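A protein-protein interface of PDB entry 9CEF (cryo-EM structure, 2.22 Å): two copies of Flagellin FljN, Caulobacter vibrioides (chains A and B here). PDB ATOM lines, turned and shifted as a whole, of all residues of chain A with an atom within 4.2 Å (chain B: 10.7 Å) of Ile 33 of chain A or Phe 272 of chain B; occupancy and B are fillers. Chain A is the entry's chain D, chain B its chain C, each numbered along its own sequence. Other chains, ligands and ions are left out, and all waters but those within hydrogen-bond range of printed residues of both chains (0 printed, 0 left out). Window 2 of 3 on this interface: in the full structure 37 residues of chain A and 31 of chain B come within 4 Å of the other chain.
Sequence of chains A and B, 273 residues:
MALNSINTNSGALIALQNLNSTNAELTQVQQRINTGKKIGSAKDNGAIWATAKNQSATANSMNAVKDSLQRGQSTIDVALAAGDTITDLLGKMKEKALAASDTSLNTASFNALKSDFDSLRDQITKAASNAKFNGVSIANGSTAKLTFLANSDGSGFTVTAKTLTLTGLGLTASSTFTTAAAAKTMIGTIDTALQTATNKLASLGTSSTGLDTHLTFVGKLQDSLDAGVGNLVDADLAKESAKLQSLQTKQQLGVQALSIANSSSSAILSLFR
The side-chain hydroxyl of Ser 5 of chain B is in hydrogen-bond range of the backbone NH of Asn 7 of chain B. O of Gln 31 of chain A lies within hydrogen-bond range of OG1 of Thr 35 of chain A, 3.0 Å away.
Of the 12 printed residues of chain B, 6 touch a printed residue of chain A. Of the 11 printed residues of chain A, 5 touch a printed residue of chain B. Hydrophobic or aromatic side chains of chain A that line the printed part of chain B: Ile 33 and Leu 237. Along chain A the printed residues that touch a printed residue of chain B span positions 33 to 241. Among the printed residues, 10 pairs touch across the chains.
The side-chain amide nitrogen (ND2) of Asn 7 of chain B sits at hydrogen-bond distance from the backbone carbonyl oxygen (O) of Thr 35 of chain A, at 3.3 Å. ND2 of Asn 7 of chain B lies within hydrogen-bond range of O of Gly 36 of chain A (3.0 Å). O of Asn 4 of chain B lies within hydrogen-bond range of N of Leu 237 of chain A (3.3 Å).
Among the printed residues, pairs that only touch across the chains: Ile 33 of chain A with Phe 272 of chain B, Gly 36 of chain A with Ile 6 of chain B, Leu 237 of chain A with Ile 6 of chain B, Leu 237 of chain A with Ile 268 of chain B, Leu 237 of chain A with Phe 272 of chain B, Ser 241 of chain A with Leu 271 of chain B and Ser 241 of chain A with Phe 272 of chain B.
No position is printed for both chains.
No residue of chain B comes within 4 Å of Val 29 of chain A. Ile 33 of chain A touches one residue of chain B. No residue of chain B comes within 4 Å of Asn 34 of chain A. Printed residues of chain B within 4 Å of Gly 36 of chain A: Ile 6 and Asn 7. Ser 241 of chain A touches two residues of chain B. Of the printed residues of chain A, Asn 4 of chain B touches Leu 237. Ser 5 of chain B touches none of the printed residues of chain A. Printed residues of chain A within 4 Å of Asn 7 of chain B: Thr 35 (3.3 Å) and Gly 36 (3.0 Å). Printed residues of chain A within 4 Å of Ile 268 of chain B: Leu 237. Of chain A, only Ile 33 (3.7 Å), Leu 237 (3.4 Å) and Ser 241 (3.6 Å) come within 4 Å of Phe 272 of chain B. The nearest printed residue of chain A that does not touch Ile 6 of chain B is Ile 33 of chain A (4.5 Å).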
ATOM      1  N   VAL A  29     -23.130  -1.923  -5.874  1.00  0.00           N
ATOM      2  CA  VAL A  29     -23.150  -0.544  -6.351  1.00  0.00           C
ATOM      3  C   VAL A  29     -24.548   0.059  -6.225  1.00  0.00           C
ATOM      4  O   VAL A  29     -24.697   1.250  -5.925  1.00  0.00           O
ATOM      5  CB  VAL A  29     -22.610  -0.466  -7.790  1.00  0.00           C
ATOM      6  CG1 VAL A  29     -22.670   0.945  -8.310  1.00  0.00           C
ATOM      7  CG2 VAL A  29     -21.189  -0.938  -7.817  1.00  0.00           C
ATOM      8  N   GLN A  30     -25.595  -0.748  -6.423  1.00  0.00           N
ATOM      9  CA  GLN A  30     -26.943  -0.214  -6.243  1.00  0.00           C
ATOM     10  C   GLN A  30     -27.200   0.182  -4.797  1.00  0.00           C
ATOM     11  O   GLN A  30     -27.834   1.210  -4.534  1.00  0.00           O
ATOM     12  CB  GLN A  30     -28.004  -1.215  -6.695  1.00  0.00           C
ATOM     13  CG  GLN A  30     -27.984  -1.569  -8.152  1.00  0.00           C
ATOM     14  CD  GLN A  30     -28.747  -2.848  -8.440  1.00  0.00           C
ATOM     15  OE1 GLN A  30     -28.453  -3.560  -9.396  1.00  0.00           O
ATOM     16  NE2 GLN A  30     -29.727  -3.149  -7.602  1.00  0.00           N
ATOM     17  N   GLN A  31     -26.706  -0.605  -3.842  1.00  0.00           N
ATOM     18  CA  GLN A  31     -26.878  -0.205  -2.447  1.00  0.00           C
ATOM     19  C   GLN A  31     -26.142   1.090  -2.140  1.00  0.00           C
ATOM     20  O   GLN A  31     -26.656   1.943  -1.408  1.00  0.00           O
ATOM     21  CB  GLN A  31     -26.412  -1.306  -1.511  1.00  0.00           C
ATOM     22  CG  GLN A  31     -27.243  -2.546  -1.570  1.00  0.00           C
ATOM     23  CD  GLN A  31     -26.617  -3.677  -0.798  1.00  0.00           C
ATOM     24  OE1 GLN A  31     -25.467  -4.034  -1.025  1.00  0.00           O
ATOM     25  NE2 GLN A  31     -27.364  -4.235   0.137  1.00  0.00           N
ATOM     26  N   ARG A  32     -24.954   1.273  -2.714  1.00  0.00           N
ATOM     27  CA  ARG A  32     -24.240   2.522  -2.466  1.00  0.00           C
ATOM     28  C   ARG A  32     -24.970   3.716  -3.059  1.00  0.00           C
ATOM     29  O   ARG A  32     -25.050   4.770  -2.427  1.00  0.00           O
ATOM     30  CB  ARG A  32     -22.824   2.453  -3.014  1.00  0.00           C
ATOM     31  CG  ARG A  32     -21.976   1.433  -2.358  1.00  0.00           C
ATOM     32  CD  ARG A  32     -20.543   1.722  -2.611  1.00  0.00           C
ATOM     33  NE  ARG A  32     -19.693   0.705  -2.022  1.00  0.00           N
ATOM     34  CZ  ARG A  32     -18.372   0.718  -2.074  1.00  0.00           C
ATOM     35  NH1 ARG A  32     -17.717   1.670  -2.711  1.00  0.00           N
ATOM     36  NH2 ARG A  32     -17.694  -0.247  -1.466  1.00  0.00           N
ATOM     37  N   ILE A  33     -25.505   3.578  -4.270  1.00  0.00           N
ATOM     38  CA  ILE A  33     -26.230   4.692  -4.871  1.00  0.00           C
ATOM     39  C   ILE A  33     -27.489   5.004  -4.077  1.00  0.00           C
ATOM     40  O   ILE A  33     -27.870   6.168  -3.923  1.00  0.00           O
ATOM     41  CB  ILE A  33     -26.553   4.398  -6.346  1.00  0.00           C
ATOM     42  CG1 ILE A  33     -25.289   4.441  -7.193  1.00  0.00           C
ATOM     43  CG2 ILE A  33     -27.596   5.357  -6.880  1.00  0.00           C
ATOM     44  CD1 ILE A  33     -25.383   3.603  -8.408  1.00  0.00           C
ATOM     45  N   ASN A  34     -28.131   3.979  -3.529  1.00  0.00           N
ATOM     46  CA  ASN A  34     -29.407   4.199  -2.866  1.00  0.00           C
ATOM     47  C   ASN A  34     -29.231   4.828  -1.491  1.00  0.00           C
ATOM     48  O   ASN A  34     -29.939   5.774  -1.141  1.00  0.00           O
ATOM     49  CB  ASN A  34     -30.156   2.882  -2.762  1.00  0.00           C
ATOM     50  CG  ASN A  34     -31.622   3.074  -2.712  1.00  0.00           C
ATOM     51  OD1 ASN A  34     -32.118   4.189  -2.563  1.00  0.00           O
ATOM     52  ND2 ASN A  34     -32.344   1.992  -2.848  1.00  0.00           N
ATOM     53  N   THR A  35     -28.301   4.318  -0.691  1.00  0.00           N
ATOM     54  CA  THR A  35     -28.107   4.893   0.633  1.00  0.00           C
ATOM     55  C   THR A  35     -27.158   6.078   0.643  1.00  0.00           C
ATOM     56  O   THR A  35     -27.178   6.856   1.597  1.00  0.00           O
ATOM     57  CB  THR A  35     -27.588   3.835   1.603  1.00  0.00           C
ATOM     58  OG1 THR A  35     -26.294   3.397   1.190  1.00  0.00           O
ATOM     59  CG2 THR A  35     -28.518   2.658   1.643  1.00  0.00           C
ATOM     60  N   GLY A  36     -26.334   6.238  -0.383  1.00  0.00           N
ATOM     61  CA  GLY A  36     -25.297   7.237  -0.315  1.00  0.00           C
ATOM     62  C   GLY A  36     -24.132   6.860   0.564  1.00  0.00           C
ATOM     63  O   GLY A  36     -23.346   7.726   0.928  1.00  0.00           O
ATOM     64  N   LEU A 237     -20.265   9.435  -5.014  1.00  0.00           N
ATOM     65  CA  LEU A 237     -21.232   9.013  -6.022  1.00  0.00           C
ATOM     66  C   LEU A 237     -20.750   9.247  -7.445  1.00  0.00           C
ATOM     67  O   LEU A 237     -21.173   8.535  -8.367  1.00  0.00           O
ATOM     68  CB  LEU A 237     -22.559   9.712  -5.770  1.00  0.00           C
ATOM     69  CG  LEU A 237     -23.272   9.000  -4.626  1.00  0.00           C
ATOM     70  CD1 LEU A 237     -24.162   9.942  -3.938  1.00  0.00           C
ATOM     71  CD2 LEU A 237     -24.070   7.837  -5.148  1.00  0.00           C
ATOM     72  N   SER A 241     -20.917   6.241 -10.327  1.00  0.00           N
ATOM     73  CA  SER A 241     -21.565   6.314 -11.640  1.00  0.00           C
ATOM     74  C   SER A 241     -20.750   5.596 -12.717  1.00  0.00           C
ATOM     75  O   SER A 241     -21.306   4.862 -13.552  1.00  0.00           O
ATOM     76  CB  SER A 241     -21.804   7.771 -12.025  1.00  0.00           C
ATOM     77  OG  SER A 241     -20.592   8.481 -12.111  1.00  0.00           O
ATOM     78  N   LEU A 244     -21.081   1.864 -12.127  1.00  0.00           N
ATOM     79  CA  LEU A 244     -22.392   1.372 -12.526  1.00  0.00           C
ATOM     80  C   LEU A 244     -22.462   1.130 -14.025  1.00  0.00           C
ATOM     81  O   LEU A 244     -22.939   0.080 -14.473  1.00  0.00           O
ATOM     82  CB  LEU A 244     -23.471   2.362 -12.103  1.00  0.00           C
ATOM     83  CG  LEU A 244     -24.870   2.129 -12.677  1.00  0.00           C
ATOM     84  CD1 LEU A 244     -25.458   0.833 -12.170  1.00  0.00           C
ATOM     85  CD2 LEU A 244     -25.778   3.284 -12.356  1.00  0.00           C
ATOM     86  N   ASN B   4     -17.904  13.668  -2.938  1.00  0.00           N
ATOM     87  CA  ASN B   4     -19.110  13.861  -3.734  1.00  0.00           C
ATOM     88  C   ASN B   4     -20.286  13.203  -3.013  1.00  0.00           C
ATOM     89  O   ASN B   4     -20.974  12.337  -3.541  1.00  0.00           O
ATOM     90  CB  ASN B   4     -18.933  13.301  -5.147  1.00  0.00           C
ATOM     91  CG  ASN B   4     -17.859  14.022  -5.936  1.00  0.00           C
ATOM     92  OD1 ASN B   4     -18.118  15.045  -6.558  1.00  0.00           O
ATOM     93  ND2 ASN B   4     -16.654  13.484  -5.924  1.00  0.00           N
ATOM     94  N   SER B   5     -20.489  13.618  -1.769  1.00  0.00           N
ATOM     95  CA  SER B   5     -21.441  13.003  -0.862  1.00  0.00           C
ATOM     96  C   SER B   5     -22.822  13.636  -0.979  1.00  0.00           C
ATOM     97  O   SER B   5     -22.959  14.834  -1.220  1.00  0.00           O
ATOM     98  CB  SER B   5     -20.929  13.124   0.573  1.00  0.00           C
ATOM     99  OG  SER B   5     -21.948  12.905   1.523  1.00  0.00           O
ATOM    100  N   ILE B   6     -23.850  12.813  -0.797  1.00  0.00           N
ATOM    101  CA  ILE B   6     -25.221  13.298  -0.692  1.00  0.00           C
ATOM    102  C   ILE B   6     -25.755  13.273   0.724  1.00  0.00           C
ATOM    103  O   ILE B   6     -26.894  13.709   0.940  1.00  0.00           O
ATOM    104  CB  ILE B   6     -26.175  12.512  -1.612  1.00  0.00           C
ATOM    105  CG1 ILE B   6     -26.214  11.044  -1.194  1.00  0.00           C
ATOM    106  CG2 ILE B   6     -25.793  12.719  -3.054  1.00  0.00           C
ATOM    107  CD1 ILE B   6     -27.120  10.191  -2.015  1.00  0.00           C
ATOM    108  N   ASN B   7     -25.001  12.760   1.687  1.00  0.00           N
ATOM    109  CA  ASN B   7     -25.467  12.689   3.061  1.00  0.00           C
ATOM    110  C   ASN B   7     -24.920  13.792   3.943  1.00  0.00           C
ATOM    111  O   ASN B   7     -25.525  14.101   4.969  1.00  0.00           O
ATOM    112  CB  ASN B   7     -25.097  11.340   3.679  1.00  0.00           C
ATOM    113  CG  ASN B   7     -25.856  10.200   3.071  1.00  0.00           C
ATOM    114  OD1 ASN B   7     -27.048  10.298   2.838  1.00  0.00           O
ATOM    115  ND2 ASN B   7     -25.172   9.111   2.812  1.00  0.00           N
ATOM    116  N   SER B 265     -25.018  19.153  -4.026  1.00  0.00           N
ATOM    117  CA  SER B 265     -25.504  17.804  -4.282  1.00  0.00           C
ATOM    118  C   SER B 265     -26.167  17.692  -5.646  1.00  0.00           C
ATOM    119  O   SER B 265     -26.097  16.637  -6.280  1.00  0.00           O
ATOM    120  CB  SER B 265     -26.484  17.380  -3.188  1.00  0.00           C
ATOM    121  OG  SER B 265     -27.494  18.358  -3.003  1.00  0.00           O
ATOM    122  N   SER B 266     -26.792  18.767  -6.115  1.00  0.00           N
ATOM    123  CA  SER B 266     -27.537  18.710  -7.362  1.00  0.00           C
ATOM    124  C   SER B 266     -26.629  18.444  -8.553  1.00  0.00           C
ATOM    125  O   SER B 266     -27.090  17.944  -9.582  1.00  0.00           O
ATOM    126  CB  SER B 266     -28.314  20.008  -7.558  1.00  0.00           C
ATOM    127  OG  SER B 266     -27.566  20.949  -8.299  1.00  0.00           O
ATOM    128  N   ALA B 267     -25.345  18.778  -8.441  1.00  0.00           N
ATOM    129  CA  ALA B 267     -24.429  18.511  -9.538  1.00  0.00           C
ATOM    130  C   ALA B 267     -24.302  17.024  -9.818  1.00  0.00           C
ATOM    131  O   ALA B 267     -24.103  16.630 -10.968  1.00  0.00           O
ATOM    132  CB  ALA B 267     -23.060  19.112  -9.233  1.00  0.00           C
ATOM    133  N   ILE B 268     -24.439  16.184  -8.793  1.00  0.00           N
ATOM    134  CA  ILE B 268     -24.234  14.751  -8.984  1.00  0.00           C
ATOM    135  C   ILE B 268     -25.399  14.103  -9.719  1.00  0.00           C
ATOM    136  O   ILE B 268     -25.238  13.036 -10.316  1.00  0.00           O
ATOM    137  CB  ILE B 268     -23.961  14.073  -7.630  1.00  0.00           C
ATOM    138  CG1 ILE B 268     -22.877  13.022  -7.805  1.00  0.00           C
ATOM    139  CG2 ILE B 268     -25.218  13.457  -7.050  1.00  0.00           C
ATOM    140  CD1 ILE B 268     -21.559  13.606  -8.203  1.00  0.00           C
ATOM    141  N   LEU B 269     -26.576  14.732  -9.713  1.00  0.00           N
ATOM    142  CA  LEU B 269     -27.740  14.128 -10.356  1.00  0.00           C
ATOM    143  C   LEU B 269     -27.532  13.958 -11.846  1.00  0.00           C
ATOM    144  O   LEU B 269     -28.128  13.071 -12.460  1.00  0.00           O
ATOM    145  CB  LEU B 269     -28.981  14.980 -10.113  1.00  0.00           C
ATOM    146  CG  LEU B 269     -29.862  14.686  -8.908  1.00  0.00           C
ATOM    147  CD1 LEU B 269     -31.123  15.510  -9.014  1.00  0.00           C
ATOM    148  CD2 LEU B 269     -30.190  13.213  -8.828  1.00  0.00           C
ATOM    149  N   SER B 270     -26.693  14.801 -12.440  1.00  0.00           N
ATOM    150  CA  SER B 270     -26.467  14.757 -13.877  1.00  0.00           C
ATOM    151  C   SER B 270     -25.808  13.458 -14.308  1.00  0.00           C
ATOM    152  O   SER B 270     -26.026  12.997 -15.431  1.00  0.00           O
ATOM    153  CB  SER B 270     -25.611  15.946 -14.284  1.00  0.00           C
ATOM    154  OG  SER B 270     -26.057  17.116 -13.624  1.00  0.00           O
ATOM    155  N   LEU B 271     -25.016  12.844 -13.431  1.00  0.00           N
ATOM    156  CA  LEU B 271     -24.266  11.652 -13.793  1.00  0.00           C
ATOM    157  C   LEU B 271     -25.118  10.398 -13.796  1.00  0.00           C
ATOM    158  O   LEU B 271     -24.649   9.353 -14.248  1.00  0.00           O
ATOM    159  CB  LEU B 271     -23.090  11.458 -12.845  1.00  0.00           C
ATOM    160  CG  LEU B 271     -21.994  12.514 -12.922  1.00  0.00           C
ATOM    161  CD1 LEU B 271     -21.121  12.467 -11.684  1.00  0.00           C
ATOM    162  CD2 LEU B 271     -21.164  12.343 -14.184  1.00  0.00           C
ATOM    163  N   PHE B 272     -26.345  10.476 -13.312  1.00  0.00           N
ATOM    164  CA  PHE B 272     -27.181   9.302 -13.164  1.00  0.00           C
ATOM    165  C   PHE B 272     -28.440   9.460 -14.003  1.00  0.00           C
ATOM    166  O   PHE B 272     -28.891   8.518 -14.644  1.00  0.00           O
ATOM    167  CB  PHE B 272     -27.526   9.101 -11.693  1.00  0.00           C
ATOM    168  CG  PHE B 272     -26.396   8.558 -10.883  1.00  0.00           C
ATOM    169  CD1 PHE B 272     -26.044   7.232 -10.962  1.00  0.00           C
ATOM    170  CD2 PHE B 272     -25.659   9.392 -10.068  1.00  0.00           C
ATOM    171  CE1 PHE B 272     -25.003   6.748 -10.230  1.00  0.00           C
ATOM    172  CE2 PHE B 272     -24.621   8.911  -9.338  1.00  0.00           C
ATOM    173  CZ  PHE B 272     -24.291   7.587  -9.414  1.00  0.00           C
